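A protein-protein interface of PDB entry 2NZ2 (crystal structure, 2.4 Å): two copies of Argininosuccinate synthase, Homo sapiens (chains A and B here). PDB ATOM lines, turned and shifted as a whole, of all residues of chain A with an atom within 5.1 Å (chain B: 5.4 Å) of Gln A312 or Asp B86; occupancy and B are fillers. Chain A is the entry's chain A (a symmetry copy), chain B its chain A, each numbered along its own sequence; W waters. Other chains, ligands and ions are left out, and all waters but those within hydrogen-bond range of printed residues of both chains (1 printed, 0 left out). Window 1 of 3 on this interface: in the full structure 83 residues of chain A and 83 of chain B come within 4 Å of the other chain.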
ATOM      1  N   SER A  80      19.155 -11.666  -5.592  1.00  0.00           N
ATOM      2  CA  SER A  80      19.333 -12.552  -6.764  1.00  0.00           C
ATOM      3  C   SER A  80      20.016 -13.894  -6.522  1.00  0.00           C
ATOM      4  O   SER A  80      19.810 -14.812  -7.295  1.00  0.00           O
ATOM      5  CB  SER A  80      20.051 -11.819  -7.896  1.00  0.00           C
ATOM      6  OG  SER A  80      21.447 -12.013  -7.827  1.00  0.00           O
ATOM      7  N   SER A  81      20.828 -13.992  -5.466  1.00  0.00           N
ATOM      8  CA  SER A  81      21.716 -15.157  -5.184  1.00  0.00           C
ATOM      9  C   SER A  81      22.544 -15.667  -6.371  1.00  0.00           C
ATOM     10  O   SER A  81      22.752 -16.884  -6.496  1.00  0.00           O
ATOM     11  CB  SER A  81      20.926 -16.337  -4.619  1.00  0.00           C
ATOM     12  OG  SER A  81      19.944 -15.903  -3.687  1.00  0.00           O
ATOM     13  N   TYR A 292      26.929 -13.057   0.258  1.00  0.00           N
ATOM     14  CA  TYR A 292      26.586 -14.016  -0.765  1.00  0.00           C
ATOM     15  C   TYR A 292      26.237 -15.363  -0.121  1.00  0.00           C
ATOM     16  O   TYR A 292      25.219 -15.979  -0.427  1.00  0.00           O
ATOM     17  CB  TYR A 292      27.755 -14.221  -1.749  1.00  0.00           C
ATOM     18  CG  TYR A 292      27.504 -15.432  -2.654  1.00  0.00           C
ATOM     19  CD1 TYR A 292      26.572 -15.352  -3.690  1.00  0.00           C
ATOM     20  CD2 TYR A 292      28.167 -16.648  -2.450  1.00  0.00           C
ATOM     21  CE1 TYR A 292      26.295 -16.419  -4.492  1.00  0.00           C
ATOM     22  CE2 TYR A 292      27.913 -17.743  -3.264  1.00  0.00           C
ATOM     23  CZ  TYR A 292      26.952 -17.612  -4.281  1.00  0.00           C
ATOM     24  OH  TYR A 292      26.651 -18.646  -5.135  1.00  0.00           O
ATOM     25  N   LEU A 296      22.356 -16.964   0.878  1.00  0.00           N
ATOM     26  CA  LEU A 296      22.079 -18.286   0.298  1.00  0.00           C
ATOM     27  C   LEU A 296      21.543 -19.183   1.369  1.00  0.00           C
ATOM     28  O   LEU A 296      20.553 -19.903   1.162  1.00  0.00           O
ATOM     29  CB  LEU A 296      23.381 -18.878  -0.261  1.00  0.00           C
ATOM     30  CG  LEU A 296      23.583 -19.584  -1.606  1.00  0.00           C
ATOM     31  CD1 LEU A 296      22.765 -19.013  -2.756  1.00  0.00           C
ATOM     32  CD2 LEU A 296      25.062 -19.544  -1.946  1.00  0.00           C
ATOM     33  N   GLU A 299      17.892 -17.795   2.482  1.00  0.00           N
ATOM     34  CA  GLU A 299      16.826 -18.081   1.501  1.00  0.00           C
ATOM     35  C   GLU A 299      16.524 -19.568   1.391  1.00  0.00           C
ATOM     36  O   GLU A 299      15.361 -19.960   1.320  1.00  0.00           O
ATOM     37  CB  GLU A 299      16.968 -17.391   0.124  1.00  0.00           C
ATOM     38  CG  GLU A 299      18.190 -17.663  -0.628  1.00  0.00           C
ATOM     39  CD  GLU A 299      18.040 -17.478  -2.148  1.00  0.00           C
ATOM     40  OE1 GLU A 299      18.791 -18.163  -2.874  1.00  0.00           O
ATOM     41  OE2 GLU A 299      17.214 -16.668  -2.613  1.00  0.00           O
ATOM     42  N   VAL A 307       9.791 -22.843  -5.639  1.00  0.00           N
ATOM     43  CA  VAL A 307       9.960 -21.410  -5.876  1.00  0.00           C
ATOM     44  C   VAL A 307      11.449 -21.152  -6.174  1.00  0.00           C
ATOM     45  O   VAL A 307      11.783 -20.446  -7.129  1.00  0.00           O
ATOM     46  CB  VAL A 307       9.360 -20.503  -4.735  1.00  0.00           C
ATOM     47  CG1 VAL A 307       9.675 -19.023  -4.976  1.00  0.00           C
ATOM     48  CG2 VAL A 307       7.836 -20.681  -4.644  1.00  0.00           C
ATOM     49  N   ARG A 308      12.327 -21.813  -5.418  1.00  0.00           N
ATOM     50  CA  ARG A 308      13.765 -21.556  -5.477  1.00  0.00           C
ATOM     51  C   ARG A 308      14.435 -21.747  -6.842  1.00  0.00           C
ATOM     52  O   ARG A 308      15.268 -20.938  -7.230  1.00  0.00           O
ATOM     53  CB  ARG A 308      14.480 -22.376  -4.416  1.00  0.00           C
ATOM     54  CG  ARG A 308      15.829 -21.813  -4.073  1.00  0.00           C
ATOM     55  CD  ARG A 308      16.682 -22.826  -3.341  1.00  0.00           C
ATOM     56  NE  ARG A 308      18.006 -22.288  -3.056  1.00  0.00           N
ATOM     57  CZ  ARG A 308      19.047 -22.341  -3.886  1.00  0.00           C
ATOM     58  NH1 ARG A 308      18.942 -22.898  -5.096  1.00  0.00           N
ATOM     59  NH2 ARG A 308      20.207 -21.801  -3.511  1.00  0.00           N
ATOM     60  N   LYS A 309      14.077 -22.813  -7.560  1.00  0.00           N
ATOM     61  CA  LYS A 309      14.682 -23.115  -8.861  1.00  0.00           C
ATOM     62  C   LYS A 309      14.217 -22.191  -9.966  1.00  0.00           C
ATOM     63  O   LYS A 309      14.958 -21.920 -10.907  1.00  0.00           O
ATOM     64  CB  LYS A 309      14.404 -24.559  -9.292  1.00  0.00           C
ATOM     65  CG  LYS A 309      14.277 -25.527  -8.147  1.00  0.00           C
ATOM     66  CD  LYS A 309      13.070 -26.422  -8.381  1.00  0.00           C
ATOM     67  CE  LYS A 309      13.472 -27.756  -8.968  1.00  0.00           C
ATOM     68  NZ  LYS A 309      13.156 -28.851  -7.999  1.00  0.00           N
ATOM     69  N   ILE A 310      12.971 -21.759  -9.875  1.00  0.00           N
ATOM     70  CA  ILE A 310      12.410 -20.760 -10.772  1.00  0.00           C
ATOM     71  C   ILE A 310      13.072 -19.423 -10.480  1.00  0.00           C
ATOM     72  O   ILE A 310      13.469 -18.705 -11.397  1.00  0.00           O
ATOM     73  CB  ILE A 310      10.872 -20.638 -10.595  1.00  0.00           C
ATOM     74  CG1 ILE A 310      10.183 -21.964 -10.949  1.00  0.00           C
ATOM     75  CG2 ILE A 310      10.324 -19.486 -11.413  1.00  0.00           C
ATOM     76  CD1 ILE A 310       8.725 -22.096 -10.391  1.00  0.00           C
ATOM     77  N   LYS A 311      13.196 -19.110  -9.195  1.00  0.00           N
ATOM     78  CA  LYS A 311      13.799 -17.865  -8.742  1.00  0.00           C
ATOM     79  C   LYS A 311      15.273 -17.793  -9.145  1.00  0.00           C
ATOM     80  O   LYS A 311      15.764 -16.747  -9.571  1.00  0.00           O
ATOM     81  CB  LYS A 311      13.605 -17.711  -7.226  1.00  0.00           C
ATOM     82  CG  LYS A 311      14.174 -16.438  -6.634  1.00  0.00           C
ATOM     83  CD  LYS A 311      15.590 -16.635  -6.146  1.00  0.00           C
ATOM     84  CE  LYS A 311      16.332 -15.314  -5.985  1.00  0.00           C
ATOM     85  NZ  LYS A 311      17.675 -15.531  -5.360  1.00  0.00           N
ATOM     86  N   GLN A 312      15.967 -18.914  -9.048  1.00  0.00           N
ATOM     87  CA  GLN A 312      17.391 -18.948  -9.361  1.00  0.00           C
ATOM     88  C   GLN A 312      17.687 -18.797 -10.850  1.00  0.00           C
ATOM     89  O   GLN A 312      18.789 -18.384 -11.230  1.00  0.00           O
ATOM     90  CB  GLN A 312      18.048 -20.213  -8.786  1.00  0.00           C
ATOM     91  CG  GLN A 312      18.213 -20.194  -7.269  1.00  0.00           C
ATOM     92  CD  GLN A 312      19.230 -19.185  -6.801  1.00  0.00           C
ATOM     93  OE1 GLN A 312      20.364 -19.536  -6.501  1.00  0.00           O
ATOM     94  NE2 GLN A 312      18.831 -17.922  -6.737  1.00  0.00           N
ATOM     95  N   GLY A 313      16.721 -19.169 -11.688  1.00  0.00           N
ATOM     96  CA  GLY A 313      16.819 -18.954 -13.120  1.00  0.00           C
ATOM     97  C   GLY A 313      16.727 -17.464 -13.370  1.00  0.00           C
ATOM     98  O   GLY A 313      17.427 -16.939 -14.226  1.00  0.00           O
ATOM     99  N   LEU A 314      15.852 -16.787 -12.629  1.00  0.00           N
ATOM    100  CA  LEU A 314      15.647 -15.341 -12.799  1.00  0.00           C
ATOM    101  C   LEU A 314      16.897 -14.585 -12.376  1.00  0.00           C
ATOM    102  O   LEU A 314      17.321 -13.679 -13.085  1.00  0.00           O
ATOM    103  CB  LEU A 314      14.435 -14.826 -11.995  1.00  0.00           C
ATOM    104  CG  LEU A 314      13.062 -15.406 -12.332  1.00  0.00           C
ATOM    105  CD1 LEU A 314      12.018 -15.084 -11.264  1.00  0.00           C
ATOM    106  CD2 LEU A 314      12.596 -14.959 -13.715  1.00  0.00           C
ATOM    107  N   GLY A 315      17.476 -14.974 -11.228  1.00  0.00           N
ATOM    108  CA  GLY A 315      18.748 -14.444 -10.752  1.00  0.00           C
ATOM    109  C   GLY A 315      19.871 -14.581 -11.769  1.00  0.00           C
ATOM    110  O   GLY A 315      20.603 -13.615 -12.044  1.00  0.00           O
ATOM    111  N   LEU A 316      19.996 -15.778 -12.343  1.00  0.00           N
ATOM    112  CA  LEU A 316      20.972 -16.027 -13.387  1.00  0.00           C
ATOM    113  C   LEU A 316      20.774 -15.021 -14.498  1.00  0.00           C
ATOM    114  O   LEU A 316      21.742 -14.494 -15.037  1.00  0.00           O
ATOM    115  CB  LEU A 316      20.839 -17.448 -13.959  1.00  0.00           C
ATOM    116  CG  LEU A 316      21.660 -18.568 -13.311  1.00  0.00           C
ATOM    117  CD1 LEU A 316      21.610 -19.868 -14.121  1.00  0.00           C
ATOM    118  CD2 LEU A 316      23.129 -18.120 -13.077  1.00  0.00           C
ATOM    119  N   LEU B  83      26.408 -27.540  -8.760  1.00  0.00           N
ATOM    120  CA  LEU B  83      26.205 -27.827  -7.334  1.00  0.00           C
ATOM    121  C   LEU B  83      24.696 -27.949  -7.081  1.00  0.00           C
ATOM    122  O   LEU B  83      23.913 -27.114  -7.541  1.00  0.00           O
ATOM    123  CB  LEU B  83      26.790 -26.692  -6.477  1.00  0.00           C
ATOM    124  CG  LEU B  83      28.292 -26.319  -6.552  1.00  0.00           C
ATOM    125  CD1 LEU B  83      28.624 -24.968  -5.956  1.00  0.00           C
ATOM    126  CD2 LEU B  83      29.177 -27.342  -5.895  1.00  0.00           C
ATOM    127  N   TYR B  84      24.270 -28.983  -6.368  1.00  0.00           N
ATOM    128  CA  TYR B  84      22.866 -29.073  -6.002  1.00  0.00           C
ATOM    129  C   TYR B  84      22.524 -27.895  -5.147  1.00  0.00           C
ATOM    130  O   TYR B  84      23.135 -27.694  -4.099  1.00  0.00           O
ATOM    131  CB  TYR B  84      22.553 -30.351  -5.236  1.00  0.00           C
ATOM    132  CG  TYR B  84      21.088 -30.460  -4.871  1.00  0.00           C
ATOM    133  CD1 TYR B  84      20.123 -30.662  -5.859  1.00  0.00           C
ATOM    134  CD2 TYR B  84      20.671 -30.359  -3.549  1.00  0.00           C
ATOM    135  CE1 TYR B  84      18.757 -30.756  -5.540  1.00  0.00           C
ATOM    136  CE2 TYR B  84      19.310 -30.459  -3.207  1.00  0.00           C
ATOM    137  CZ  TYR B  84      18.360 -30.651  -4.212  1.00  0.00           C
ATOM    138  OH  TYR B  84      17.031 -30.756  -3.893  1.00  0.00           O
ATOM    139  N   GLU B  85      21.557 -27.111  -5.597  1.00  0.00           N
ATOM    140  CA  GLU B  85      21.097 -25.910  -4.872  1.00  0.00           C
ATOM    141  C   GLU B  85      22.244 -24.966  -4.460  1.00  0.00           C
ATOM    142  O   GLU B  85      22.249 -24.410  -3.370  1.00  0.00           O
ATOM    143  CB  GLU B  85      20.212 -26.291  -3.682  1.00  0.00           C
ATOM    144  CG  GLU B  85      18.878 -26.866  -4.084  1.00  0.00           C
ATOM    145  CD  GLU B  85      17.993 -27.247  -2.901  1.00  0.00           C
ATOM    146  OE1 GLU B  85      18.495 -27.676  -1.834  1.00  0.00           O
ATOM    147  OE2 GLU B  85      16.770 -27.120  -3.041  1.00  0.00           O
ATOM    148  N   ASP B  86      23.212 -24.824  -5.362  1.00  0.00           N
ATOM    149  CA  ASP B  86      24.331 -23.883  -5.266  1.00  0.00           C
ATOM    150  C   ASP B  86      25.330 -24.160  -4.164  1.00  0.00           C
ATOM    151  O   ASP B  86      26.183 -23.303  -3.889  1.00  0.00           O
ATOM    152  CB  ASP B  86      23.845 -22.448  -5.145  1.00  0.00           C
ATOM    153  CG  ASP B  86      22.833 -22.095  -6.192  1.00  0.00           C
ATOM    154  OD1 ASP B  86      23.233 -21.842  -7.344  1.00  0.00           O
ATOM    155  OD2 ASP B  86      21.628 -22.060  -5.848  1.00  0.00           O
ATOM    156  N   ARG B  87      25.227 -25.335  -3.528  1.00  0.00           N
ATOM    157  CA  ARG B  87      26.082 -25.660  -2.368  1.00  0.00           C
ATOM    158  C   ARG B  87      26.596 -27.085  -2.292  1.00  0.00           C
ATOM    159  O   ARG B  87      27.747 -27.302  -1.953  1.00  0.00           O
ATOM    160  CB  ARG B  87      25.358 -25.338  -1.063  1.00  0.00           C
ATOM    161  CG  ARG B  87      25.254 -23.850  -0.713  1.00  0.00           C
ATOM    162  CD  ARG B  87      23.914 -23.637  -0.097  1.00  0.00           C
ATOM    163  NE  ARG B  87      23.996 -23.066   1.232  1.00  0.00           N
ATOM    164  CZ  ARG B  87      23.068 -23.218   2.168  1.00  0.00           C
ATOM    165  NH1 ARG B  87      21.988 -23.934   1.936  1.00  0.00           N
ATOM    166  NH2 ARG B  87      23.240 -22.660   3.347  1.00  0.00           N
ATOM    167  N   TYR B  88      25.744 -28.047  -2.597  1.00  0.00           N
ATOM    168  CA  TYR B  88      26.051 -29.467  -2.408  1.00  0.00           C
ATOM    169  C   TYR B  88      26.766 -30.094  -3.603  1.00  0.00           C
ATOM    170  O   TYR B  88      26.246 -30.114  -4.713  1.00  0.00           O
ATOM    171  CB  TYR B  88      24.751 -30.232  -2.090  1.00  0.00           C
ATOM    172  CG  TYR B  88      24.925 -31.697  -1.771  1.00  0.00           C
ATOM    173  CD1 TYR B  88      25.939 -32.138  -0.915  1.00  0.00           C
ATOM    174  CD2 TYR B  88      24.054 -32.658  -2.310  1.00  0.00           C
ATOM    175  CE1 TYR B  88      26.090 -33.493  -0.624  1.00  0.00           C
ATOM    176  CE2 TYR B  88      24.206 -34.014  -2.016  1.00  0.00           C
ATOM    177  CZ  TYR B  88      25.222 -34.412  -1.180  1.00  0.00           C
ATOM    178  OH  TYR B  88      25.370 -35.731  -0.886  1.00  0.00           O
HETATM  179  O   HOH W   1      24.623 -18.843  -6.834  1.00  0.00           O
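NE2 of Gln A312 is in hydrogen-bond range of O of Ser A80 (3.3 Å).
The side-chain carboxylate of Glu A299 is in salt-bridge range of the guanidinium group of Arg A308 (3.96 Å).
The side-chain amino group of Lys A311 lies close to the side-chain amide nitrogen of Gln A312 (3.0 Å).
No position is printed for both chains.
Of the 3 pairs that touch across the chains among the printed residues, none has its exchanged pair printed and touching as well.
Water W1 lies within hydrogen-bond range of the side-chain hydroxyl of Tyr A292 (2.7 Å), the backbone carbonyl oxygen of Ser A81 (2.7 Å) and the side-chain carboxylate of Asp B86 (3.3 Å).
Of the printed residues of chain B, Arg A308 touches Glu B85 and Asp B86.
Of the printed residues of chain B, Gln A312 touches Asp B86 (2.9 Å).
Of the printed residues of chain A, Glu B85 touches Arg A308 (3.3 Å).
The nearest printed residue of chain B that does not touch Gln A312 is Glu B85 (6.1 Å).
The nearest printed residue of chain A that does not touch Glu B85 is Leu A296 (5.3 Å).
Along chain A the printed residues that touch a printed residue of chain B span positions 308 to 312.
Among the printed residues, Asp or Glu carboxylates within 4 Å of a Lys or Arg side-chain nitrogen of the other chain: Arg A308 with Asp B86 (2.7 Å).
The guanidinium group (NH2) of Arg A308 lies within hydrogen-bond range of the backbone carbonyl oxygen (O) of Glu B85 (3.3 Å).
OD2 of Asp B86 is in salt-bridge range of NH2 of Arg A308.
The side-chain amide oxygen (OE1) of Gln A312 sits close to the side-chain carboxylate (OD2) of Asp B86, at 2.9 Å.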
